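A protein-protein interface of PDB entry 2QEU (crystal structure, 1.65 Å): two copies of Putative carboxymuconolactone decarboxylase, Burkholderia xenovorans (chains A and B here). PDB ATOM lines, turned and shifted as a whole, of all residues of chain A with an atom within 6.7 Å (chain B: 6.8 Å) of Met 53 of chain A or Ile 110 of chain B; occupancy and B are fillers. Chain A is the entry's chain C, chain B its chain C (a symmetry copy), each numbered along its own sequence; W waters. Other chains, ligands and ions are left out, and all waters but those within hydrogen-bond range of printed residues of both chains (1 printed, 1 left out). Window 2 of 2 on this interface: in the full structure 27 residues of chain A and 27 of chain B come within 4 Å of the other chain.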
ATOM      1  N   TYR A  46      -3.362   6.540 -12.371  1.00  0.00           N
ATOM      2  CA  TYR A  46      -3.801   5.232 -12.844  1.00  0.00           C
ATOM      3  C   TYR A  46      -3.407   4.993 -14.292  1.00  0.00           C
ATOM      4  O   TYR A  46      -2.925   3.913 -14.669  1.00  0.00           O
ATOM      5  CB  TYR A  46      -5.291   5.081 -12.689  1.00  0.00           C
ATOM      6  CG  TYR A  46      -5.815   3.751 -13.251  1.00  0.00           C
ATOM      7  CD1 TYR A  46      -5.658   2.562 -12.539  1.00  0.00           C
ATOM      8  CD2 TYR A  46      -6.371   3.688 -14.513  1.00  0.00           C
ATOM      9  CE1 TYR A  46      -6.103   1.344 -13.045  1.00  0.00           C
ATOM     10  CE2 TYR A  46      -6.865   2.528 -15.007  1.00  0.00           C
ATOM     11  CZ  TYR A  46      -6.664   1.322 -14.284  1.00  0.00           C
ATOM     12  OH  TYR A  46      -7.168   0.115 -14.754  1.00  0.00           O
ATOM     13  N   ARG A  48      -0.949   6.449 -15.910  1.00  0.00           N
ATOM     14  CA  ARG A  48       0.507   6.259 -15.949  1.00  0.00           C
ATOM     15  C   ARG A  48       0.857   4.803 -15.660  1.00  0.00           C
ATOM     16  O   ARG A  48       1.670   4.193 -16.367  1.00  0.00           O
ATOM     17  CB  ARG A  48       1.188   7.164 -14.927  1.00  0.00           C
ATOM     18  CG  ARG A  48       1.115   8.627 -15.310  1.00  0.00           C
ATOM     19  CD  ARG A  48       1.802   9.533 -14.298  1.00  0.00           C
ATOM     20  NE  ARG A  48       3.237   9.357 -14.273  1.00  0.00           N
ATOM     21  CZ  ARG A  48       4.091   9.959 -15.084  1.00  0.00           C
ATOM     22  NH1 ARG A  48       3.683  10.830 -16.022  1.00  0.00           N
ATOM     23  NH2 ARG A  48       5.369   9.705 -14.944  1.00  0.00           N
ATOM     24  N   MET A  49       0.208   4.270 -14.634  1.00  0.00           N
ATOM     25  CA  MET A  49       0.413   2.890 -14.194  1.00  0.00           C
ATOM     26  C   MET A  49       0.042   1.935 -15.351  1.00  0.00           C
ATOM     27  O   MET A  49       0.770   0.999 -15.695  1.00  0.00           O
ATOM     28  CB  MET A  49      -0.413   2.553 -12.908  1.00  0.00           C
ATOM     29  CG  MET A  49      -0.028   1.203 -12.337  1.00  0.00           C
ATOM     30  SD  MET A  49      -0.956   0.908 -10.689  1.00  0.00           S
ATOM     31  CE  MET A  49      -2.682   0.456 -11.464  1.00  0.00           C
ATOM     32  N   ARG A  50      -1.110   2.150 -15.935  1.00  0.00           N
ATOM     33  CA  ARG A  50      -1.613   1.305 -17.013  1.00  0.00           C
ATOM     34  C   ARG A  50      -0.692   1.370 -18.238  1.00  0.00           C
ATOM     35  O   ARG A  50      -0.494   0.354 -18.916  1.00  0.00           O
ATOM     36  CB  ARG A  50      -2.993   1.855 -17.412  1.00  0.00           C
ATOM     37  CG  ARG A  50      -3.845   0.878 -18.177  1.00  0.00           C
ATOM     38  CD  ARG A  50      -5.140   1.569 -18.641  1.00  0.00           C
ATOM     39  NE  ARG A  50      -6.045   0.538 -19.109  1.00  0.00           N
ATOM     40  CZ  ARG A  50      -6.041   0.011 -20.340  1.00  0.00           C
ATOM     41  NH1 ARG A  50      -5.194   0.422 -21.259  1.00  0.00           N
ATOM     42  NH2 ARG A  50      -6.870  -0.999 -20.605  1.00  0.00           N
ATOM     43  N   THR A  51      -0.198   2.570 -18.504  1.00  0.00           N
ATOM     44  CA  THR A  51       0.711   2.807 -19.656  1.00  0.00           C
ATOM     45  C   THR A  51       1.984   1.949 -19.554  1.00  0.00           C
ATOM     46  O   THR A  51       2.380   1.334 -20.571  1.00  0.00           O
ATOM     47  CB  THR A  51       1.002   4.289 -19.852  1.00  0.00           C
ATOM     48  OG1 THR A  51      -0.220   4.941 -20.180  1.00  0.00           O
ATOM     49  CG2 THR A  51       1.988   4.537 -20.987  1.00  0.00           C
ATOM     50  N   THR A  52       2.599   1.887 -18.352  1.00  0.00           N
ATOM     51  CA  THR A  52       3.744   1.017 -18.173  1.00  0.00           C
ATOM     52  C   THR A  52       3.348  -0.465 -18.186  1.00  0.00           C
ATOM     53  O   THR A  52       4.009  -1.285 -18.847  1.00  0.00           O
ATOM     54  CB  THR A  52       4.605   1.394 -16.920  1.00  0.00           C
ATOM     55  OG1 THR A  52       5.679   0.457 -16.824  1.00  0.00           O
ATOM     56  CG2 THR A  52       3.847   1.413 -15.635  1.00  0.00           C
ATOM     57  N   MET A  53       2.267  -0.804 -17.509  1.00  0.00           N
ATOM     58  CA  MET A  53       1.820  -2.193 -17.453  1.00  0.00           C
ATOM     59  C   MET A  53       1.536  -2.803 -18.813  1.00  0.00           C
ATOM     60  O   MET A  53       1.846  -3.974 -19.043  1.00  0.00           O
ATOM     61  CB  MET A  53       0.616  -2.334 -16.542  1.00  0.00           C
ATOM     62  CG  MET A  53       0.973  -2.273 -15.093  1.00  0.00           C
ATOM     63  SD  MET A  53      -0.686  -2.381 -14.094  1.00  0.00           S
ATOM     64  CE  MET A  53       0.127  -2.512 -12.290  1.00  0.00           C
ATOM     65  N   LEU A  54       0.953  -2.008 -19.713  1.00  0.00           N
ATOM     66  CA  LEU A  54       0.528  -2.497 -21.000  1.00  0.00           C
ATOM     67  C   LEU A  54       1.432  -2.024 -22.141  1.00  0.00           C
ATOM     68  O   LEU A  54       1.023  -2.024 -23.286  1.00  0.00           O
ATOM     69  CB  LEU A  54      -0.946  -2.147 -21.196  1.00  0.00           C
ATOM     70  CG  LEU A  54      -1.956  -2.975 -20.402  1.00  0.00           C
ATOM     71  CD1 LEU A  54      -3.348  -2.344 -20.401  1.00  0.00           C
ATOM     72  CD2 LEU A  54      -1.924  -4.452 -21.008  1.00  0.00           C
ATOM     73  N   LYS A  55       2.689  -1.694 -21.826  1.00  0.00           N
ATOM     74  CA  LYS A  55       3.687  -1.413 -22.819  1.00  0.00           C
ATOM     75  C   LYS A  55       3.823  -2.574 -23.820  1.00  0.00           C
ATOM     76  O   LYS A  55       3.799  -3.759 -23.441  1.00  0.00           O
ATOM     77  CB  LYS A  55       5.011  -1.173 -22.091  1.00  0.00           C
ATOM     78  CG  LYS A  55       6.107  -0.703 -22.885  1.00  0.00           C
ATOM     79  CD  LYS A  55       7.092   0.072 -22.029  1.00  0.00           C
ATOM     80  CE  LYS A  55       7.795  -0.750 -21.005  1.00  0.00           C
ATOM     81  NZ  LYS A  55       8.445   0.167 -19.985  1.00  0.00           N
ATOM     82  N   SER A  56       3.997  -2.228 -25.091  1.00  0.00           N
ATOM     83  CA  SER A  56       4.159  -3.209 -26.169  1.00  0.00           C
ATOM     84  C   SER A  56       5.605  -3.748 -26.219  1.00  0.00           C
ATOM     85  O   SER A  56       6.529  -3.153 -25.667  1.00  0.00           O
ATOM     86  CB  SER A  56       3.886  -2.536 -27.516  1.00  0.00           C
ATOM     87  OG  SER A  56       4.852  -1.544 -27.713  1.00  0.00           O
ATOM     88  N   ALA A  61       8.656  -4.085 -23.773  1.00  0.00           N
ATOM     89  CA  ALA A  61       8.037  -5.148 -22.983  1.00  0.00           C
ATOM     90  C   ALA A  61       8.521  -6.544 -23.369  1.00  0.00           C
ATOM     91  O   ALA A  61       8.880  -6.808 -24.531  1.00  0.00           O
ATOM     92  CB  ALA A  61       6.467  -5.090 -23.061  1.00  0.00           C
ATOM     93  N   LEU A  65       1.858  -8.300 -26.024  1.00  0.00           N
ATOM     94  CA  LEU A  65       0.669  -7.531 -25.717  1.00  0.00           C
ATOM     95  C   LEU A  65      -0.594  -8.357 -25.814  1.00  0.00           C
ATOM     96  O   LEU A  65      -1.526  -8.199 -25.013  1.00  0.00           O
ATOM     97  CB  LEU A  65       0.565  -6.325 -26.653  1.00  0.00           C
ATOM     98  CG  LEU A  65      -0.522  -5.301 -26.285  1.00  0.00           C
ATOM     99  CD1 LEU A  65      -0.419  -4.772 -24.858  1.00  0.00           C
ATOM    100  CD2 LEU A  65      -0.518  -4.153 -27.371  1.00  0.00           C
ATOM    101  N   LYS A  68      -0.771 -10.093 -22.518  1.00  0.00           N
ATOM    102  CA  LYS A  68      -1.184  -9.131 -21.481  1.00  0.00           C
ATOM    103  C   LYS A  68      -2.691  -8.947 -21.488  1.00  0.00           C
ATOM    104  O   LYS A  68      -3.329  -9.112 -20.452  1.00  0.00           O
ATOM    105  CB  LYS A  68      -0.484  -7.788 -21.639  1.00  0.00           C
ATOM    106  CG  LYS A  68       1.024  -7.819 -21.560  1.00  0.00           C
ATOM    107  CD  LYS A  68       1.596  -6.448 -21.462  1.00  0.00           C
ATOM    108  CE  LYS A  68       3.072  -6.417 -21.094  1.00  0.00           C
ATOM    109  NZ  LYS A  68       3.617  -5.012 -20.925  1.00  0.00           N
ATOM    110  N   LEU A  75      -9.010 -12.214 -16.053  1.00  0.00           N
ATOM    111  CA  LEU A  75      -9.329 -11.493 -14.789  1.00  0.00           C
ATOM    112  C   LEU A  75     -10.725 -10.856 -14.838  1.00  0.00           C
ATOM    113  O   LEU A  75     -11.459 -10.907 -13.844  1.00  0.00           O
ATOM    114  CB  LEU A  75      -8.306 -10.407 -14.544  1.00  0.00           C
ATOM    115  CG  LEU A  75      -6.894 -10.895 -14.161  1.00  0.00           C
ATOM    116  CD1 LEU A  75      -5.876  -9.762 -14.172  1.00  0.00           C
ATOM    117  CD2 LEU A  75      -6.941 -11.532 -12.789  1.00  0.00           C
ATOM    118  N   ILE B  78      -4.632 -14.002  -7.272  1.00  0.00           N
ATOM    119  CA  ILE B  78      -5.908 -13.435  -6.879  1.00  0.00           C
ATOM    120  C   ILE B  78      -6.564 -14.258  -5.784  1.00  0.00           C
ATOM    121  O   ILE B  78      -7.030 -13.695  -4.790  1.00  0.00           O
ATOM    122  CB  ILE B  78      -6.852 -13.321  -8.083  1.00  0.00           C
ATOM    123  CG1 ILE B  78      -6.212 -12.516  -9.218  1.00  0.00           C
ATOM    124  CG2 ILE B  78      -8.139 -12.626  -7.671  1.00  0.00           C
ATOM    125  CD1 ILE B  78      -5.498 -11.255  -8.781  1.00  0.00           C
ATOM    126  N   GLU B 104       5.673  -9.033 -15.440  1.00  0.00           N
ATOM    127  CA  GLU B 104       4.720  -8.239 -16.250  1.00  0.00           C
ATOM    128  C   GLU B 104       3.271  -8.787 -16.161  1.00  0.00           C
ATOM    129  O   GLU B 104       2.302  -8.044 -16.074  1.00  0.00           O
ATOM    130  CB  GLU B 104       5.151  -8.162 -17.699  1.00  0.00           C
ATOM    131  CG  GLU B 104       6.407  -7.352 -17.923  1.00  0.00           C
ATOM    132  CD  GLU B 104       6.769  -7.147 -19.395  1.00  0.00           C
ATOM    133  OE1 GLU B 104       5.882  -7.300 -20.272  1.00  0.00           O
ATOM    134  OE2 GLU B 104       7.932  -6.798 -19.693  1.00  0.00           O
ATOM    135  N   GLY B 105       3.124 -10.103 -16.184  1.00  0.00           N
ATOM    136  CA  GLY B 105       1.796 -10.675 -16.077  1.00  0.00           C
ATOM    137  C   GLY B 105       1.153 -10.516 -14.693  1.00  0.00           C
ATOM    138  O   GLY B 105       0.002 -10.164 -14.591  1.00  0.00           O
ATOM    139  N   ILE B 106       1.909 -10.812 -13.615  1.00  0.00           N
ATOM    140  CA  ILE B 106       1.382 -10.698 -12.245  1.00  0.00           C
ATOM    141  C   ILE B 106       0.931  -9.258 -11.973  1.00  0.00           C
ATOM    142  O   ILE B 106      -0.078  -8.993 -11.302  1.00  0.00           O
ATOM    143  CB  ILE B 106       2.396 -11.209 -11.197  1.00  0.00           C
ATOM    144  CG1 ILE B 106       2.621 -12.728 -11.295  1.00  0.00           C
ATOM    145  CG2 ILE B 106       1.985 -10.812  -9.763  1.00  0.00           C
ATOM    146  CD1 ILE B 106       3.852 -13.219 -10.453  1.00  0.00           C
ATOM    147  N   LEU B 107       1.704  -8.281 -12.451  1.00  0.00           N
ATOM    148  CA  LEU B 107       1.311  -6.865 -12.219  1.00  0.00           C
ATOM    149  C   LEU B 107      -0.078  -6.534 -12.697  1.00  0.00           C
ATOM    150  O   LEU B 107      -0.766  -5.668 -12.158  1.00  0.00           O
ATOM    151  CB  LEU B 107       2.322  -5.924 -12.862  1.00  0.00           C
ATOM    152  CG  LEU B 107       3.695  -5.891 -12.193  1.00  0.00           C
ATOM    153  CD1 LEU B 107       4.764  -5.165 -13.077  1.00  0.00           C
ATOM    154  CD2 LEU B 107       3.636  -5.274 -10.760  1.00  0.00           C
ATOM    155  N   LEU B 108      -0.493  -7.173 -13.789  1.00  0.00           N
ATOM    156  CA  LEU B 108      -1.808  -6.885 -14.359  1.00  0.00           C
ATOM    157  C   LEU B 108      -2.940  -7.187 -13.392  1.00  0.00           C
ATOM    158  O   LEU B 108      -4.034  -6.594 -13.452  1.00  0.00           O
ATOM    159  CB  LEU B 108      -2.007  -7.699 -15.643  1.00  0.00           C
ATOM    160  CG  LEU B 108      -1.006  -7.377 -16.771  1.00  0.00           C
ATOM    161  CD1 LEU B 108      -1.184  -8.292 -18.040  1.00  0.00           C
ATOM    162  CD2 LEU B 108      -1.114  -5.865 -17.167  1.00  0.00           C
ATOM    163  N   GLY B 109      -2.711  -8.123 -12.479  1.00  0.00           N
ATOM    164  CA  GLY B 109      -3.681  -8.357 -11.405  1.00  0.00           C
ATOM    165  C   GLY B 109      -4.088  -7.142 -10.595  1.00  0.00           C
ATOM    166  O   GLY B 109      -5.188  -7.028 -10.074  1.00  0.00           O
ATOM    167  N   ILE B 110      -3.160  -6.211 -10.468  1.00  0.00           N
ATOM    168  CA  ILE B 110      -3.413  -4.980  -9.727  1.00  0.00           C
ATOM    169  C   ILE B 110      -4.554  -4.153 -10.352  1.00  0.00           C
ATOM    170  O   ILE B 110      -5.357  -3.542  -9.637  1.00  0.00           O
ATOM    171  CB  ILE B 110      -2.131  -4.133  -9.587  1.00  0.00           C
ATOM    172  CG1 ILE B 110      -1.041  -4.897  -8.781  1.00  0.00           C
ATOM    173  CG2 ILE B 110      -2.442  -2.746  -8.914  1.00  0.00           C
ATOM    174  CD1 ILE B 110       0.371  -4.254  -8.939  1.00  0.00           C
ATOM    175  N   ILE B 111      -4.623  -4.138 -11.679  1.00  0.00           N
ATOM    176  CA  ILE B 111      -5.719  -3.362 -12.342  1.00  0.00           C
ATOM    177  C   ILE B 111      -7.086  -3.839 -11.933  1.00  0.00           C
ATOM    178  O   ILE B 111      -7.979  -3.058 -11.627  1.00  0.00           O
ATOM    179  CB  ILE B 111      -5.589  -3.557 -13.881  1.00  0.00           C
ATOM    180  CG1 ILE B 111      -4.369  -2.754 -14.398  1.00  0.00           C
ATOM    181  CG2 ILE B 111      -6.875  -3.111 -14.645  1.00  0.00           C
ATOM    182  CD1 ILE B 111      -3.989  -2.933 -15.918  1.00  0.00           C
ATOM    183  N   VAL B 112      -7.250  -5.167 -11.922  1.00  0.00           N
ATOM    184  CA  VAL B 112      -8.554  -5.757 -11.706  1.00  0.00           C
ATOM    185  C   VAL B 112      -8.856  -6.030 -10.237  1.00  0.00           C
ATOM    186  O   VAL B 112      -9.997  -6.005  -9.837  1.00  0.00           O
ATOM    187  CB  VAL B 112      -8.787  -6.976 -12.601  1.00  0.00           C
ATOM    188  CG1 VAL B 112     -10.215  -7.499 -12.460  1.00  0.00           C
ATOM    189  CG2 VAL B 112      -8.478  -6.614 -14.102  1.00  0.00           C
ATOM    190  N   TYR B 113      -7.814  -6.270  -9.437  1.00  0.00           N
ATOM    191  CA  TYR B 113      -7.967  -6.787  -8.058  1.00  0.00           C
ATOM    192  C   TYR B 113      -7.163  -5.984  -7.024  1.00  0.00           C
ATOM    193  O   TYR B 113      -7.135  -6.379  -5.883  1.00  0.00           O
ATOM    194  CB  TYR B 113      -7.618  -8.281  -8.014  1.00  0.00           C
ATOM    195  CG  TYR B 113      -8.818  -9.097  -8.416  1.00  0.00           C
ATOM    196  CD1 TYR B 113      -9.818  -9.445  -7.503  1.00  0.00           C
ATOM    197  CD2 TYR B 113      -8.950  -9.548  -9.710  1.00  0.00           C
ATOM    198  CE1 TYR B 113     -10.943 -10.190  -7.916  1.00  0.00           C
ATOM    199  CE2 TYR B 113     -10.056 -10.297 -10.082  1.00  0.00           C
ATOM    200  CZ  TYR B 113     -11.032 -10.613  -9.209  1.00  0.00           C
ATOM    201  OH  TYR B 113     -12.132 -11.328  -9.652  1.00  0.00           O
ATOM    202  N   GLY B 114      -6.563  -4.862  -7.412  1.00  0.00           N
ATOM    203  CA  GLY B 114      -5.888  -3.988  -6.457  1.00  0.00           C
ATOM    204  C   GLY B 114      -4.554  -4.465  -5.995  1.00  0.00           C
ATOM    205  O   GLY B 114      -4.045  -5.512  -6.442  1.00  0.00           O
ATOM    206  N   MET B 115      -3.932  -3.668  -5.142  1.00  0.00           N
ATOM    207  CA  MET B 115      -2.562  -3.966  -4.723  1.00  0.00           C
ATOM    208  C   MET B 115      -2.405  -5.356  -4.086  1.00  0.00           C
ATOM    209  O   MET B 115      -1.378  -5.977  -4.219  1.00  0.00           O
ATOM    210  CB  MET B 115      -2.032  -2.866  -3.824  1.00  0.00           C
ATOM    211  CG  MET B 115      -0.560  -2.992  -3.403  1.00  0.00           C
ATOM    212  SD  MET B 115       0.642  -3.304  -4.877  1.00  0.00           S
ATOM    213  CE  MET B 115       0.291  -1.676  -5.923  1.00  0.00           C
ATOM    214  N   PRO B 116      -3.454  -5.859  -3.392  1.00  0.00           N
ATOM    215  CA  PRO B 116      -3.328  -7.197  -2.830  1.00  0.00           C
ATOM    216  C   PRO B 116      -3.085  -8.345  -3.824  1.00  0.00           C
ATOM    217  O   PRO B 116      -2.528  -9.380  -3.429  1.00  0.00           O
ATOM    218  CB  PRO B 116      -4.645  -7.383  -2.087  1.00  0.00           C
ATOM    219  CG  PRO B 116      -5.100  -5.957  -1.763  1.00  0.00           C
ATOM    220  CD  PRO B 116      -4.722  -5.214  -2.946  1.00  0.00           C
ATOM    221  N   ALA B 117      -3.422  -8.120  -5.119  1.00  0.00           N
ATOM    222  CA  ALA B 117      -3.099  -9.060  -6.212  1.00  0.00           C
ATOM    223  C   ALA B 117      -1.585  -9.256  -6.341  1.00  0.00           C
ATOM    224  O   ALA B 117      -1.128 -10.320  -6.806  1.00  0.00           O
ATOM    225  CB  ALA B 117      -3.679  -8.589  -7.542  1.00  0.00           C
ATOM    226  N   TRP B 118      -0.814  -8.246  -5.946  1.00  0.00           N
ATOM    227  CA  TRP B 118       0.636  -8.348  -5.772  1.00  0.00           C
ATOM    228  C   TRP B 118       1.066  -8.668  -4.338  1.00  0.00           C
ATOM    229  O   TRP B 118       1.917  -9.522  -4.081  1.00  0.00           O
ATOM    230  CB  TRP B 118       1.281  -7.055  -6.281  1.00  0.00           C
ATOM    231  CG  TRP B 118       2.715  -6.891  -5.968  1.00  0.00           C
ATOM    232  CD1 TRP B 118       3.243  -6.264  -4.879  1.00  0.00           C
ATOM    233  CD2 TRP B 118       3.778  -7.294  -6.787  1.00  0.00           C
ATOM    234  NE1 TRP B 118       4.622  -6.260  -4.973  1.00  0.00           N
ATOM    235  CE2 TRP B 118       4.979  -6.904  -6.130  1.00  0.00           C
ATOM    236  CE3 TRP B 118       3.858  -7.919  -8.028  1.00  0.00           C
ATOM    237  CZ2 TRP B 118       6.230  -7.131  -6.691  1.00  0.00           C
ATOM    238  CZ3 TRP B 118       5.109  -8.182  -8.577  1.00  0.00           C
ATOM    239  CH2 TRP B 118       6.284  -7.777  -7.906  1.00  0.00           C
ATOM    240  N   GLY B 119       0.504  -7.959  -3.398  1.00  0.00           N
ATOM    241  CA  GLY B 119       1.019  -7.814  -2.083  1.00  0.00           C
ATOM    242  C   GLY B 119       0.873  -9.085  -1.268  1.00  0.00           C
ATOM    243  O   GLY B 119       1.759  -9.433  -0.479  1.00  0.00           O
HETATM  244  O   HOH W   1       2.799  -5.434 -16.737  1.00  0.00           O
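NZ of Lys 68 of chain A lies within salt-bridge range of OE1 of Glu 104 of chain B (3.3 Å).
The backbone carbonyl oxygen of Met 53 of chain A lies within hydrogen-bond range of the side-chain amino group of Lys 68 of chain A, at 2.8 Å.
The backbone carbonyl oxygen of Lys 55 of chain A is in hydrogen-bond range of the side-chain amino group of Lys 68 of chain A (2.8 Å).
The backbone carbonyl oxygen (O) of Ser 56 of chain A lies within hydrogen-bond range of the backbone NH (N) of Ala 61 of chain A, at 3.0 Å.
CG2 of Ile 111 of chain B touches OH of Tyr 46 of chain A, at 3.2 Å.
Met 53 of chain A touches Leu 107 of chain B (CE to O, 3.3 Å).
Met 53 of chain A touches Leu 108 of chain B.
CE of Met 53 of chain A touches CD1 of Ile 110 of chain B (3.8 Å).
SD of Met 53 of chain A touches CG1 of Ile 111 of chain B, 3.7 Å away.
Glu 104 of chain B touches Ala 61 of chain A.
Lys 68 of chain A touches Leu 108 of chain B (O to CD1, 3.3 Å).
CD1 of Leu 75 of chain A touches O of Leu 108 of chain B, 3.7 Å away.
CD1 of Leu 75 of chain A touches CA of Gly 109 of chain B, at 3.8 Å.
Val 112 of chain B touches Leu 75 of chain A.
Printed residues of chain A within 4 Å of Ile 110 of chain B: Met 53 (3.8 Å).
Of the printed residues of chain A, Glu 104 of chain B touches Ala 61 (3.6 Å) and Lys 68 (3.1 Å).
Of the printed residues of chain A, Ile 111 of chain B touches Tyr 46 (3.2 Å) and Met 53 (3.7 Å).
Printed residues of chain A within 4 Å of Leu 108 of chain B: Met 53, Lys 68 and Leu 75.
Printed residues of chain B within 4 Å of Leu 75 of chain A: Ile 78 (3.8 Å), Leu 108 (3.7 Å), Gly 109 (3.8 Å) and Val 112 (3.8 Å).
Of the printed residues of chain B, Ala 61 of chain A touches Glu 104.
Leu 65 of chain A touches none of the printed residues of chain B.
Tyr 113 of chain B touches none of the printed residues of chain A.
The nearest residue of chain A that does not touch Ile 110 of chain B is Met 49 of chain A (4.1 Å).
The nearest printed residue of chain B that does not touch Leu 75 of chain A is Tyr 113 of chain B (4.1 Å).
Of the 14 printed residues of chain A, 5 touch a printed residue of chain B.
Hydrophobic or aromatic side chains of chain A within 4 Å of the printed part of chain B: Tyr 46, Met 53, Ala 61 and Leu 75.
Hydrophobic or aromatic side chains of chain B within 4 Å of the printed part of chain A: Ile 78, Leu 108, Ile 110, Ile 111 and Val 112.
No position is printed for both chains.
Water W1 lies within hydrogen-bond range of O of Glu 104 of chain B (2.7 Å) and O of Met 53 of chain A (2.9 Å).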
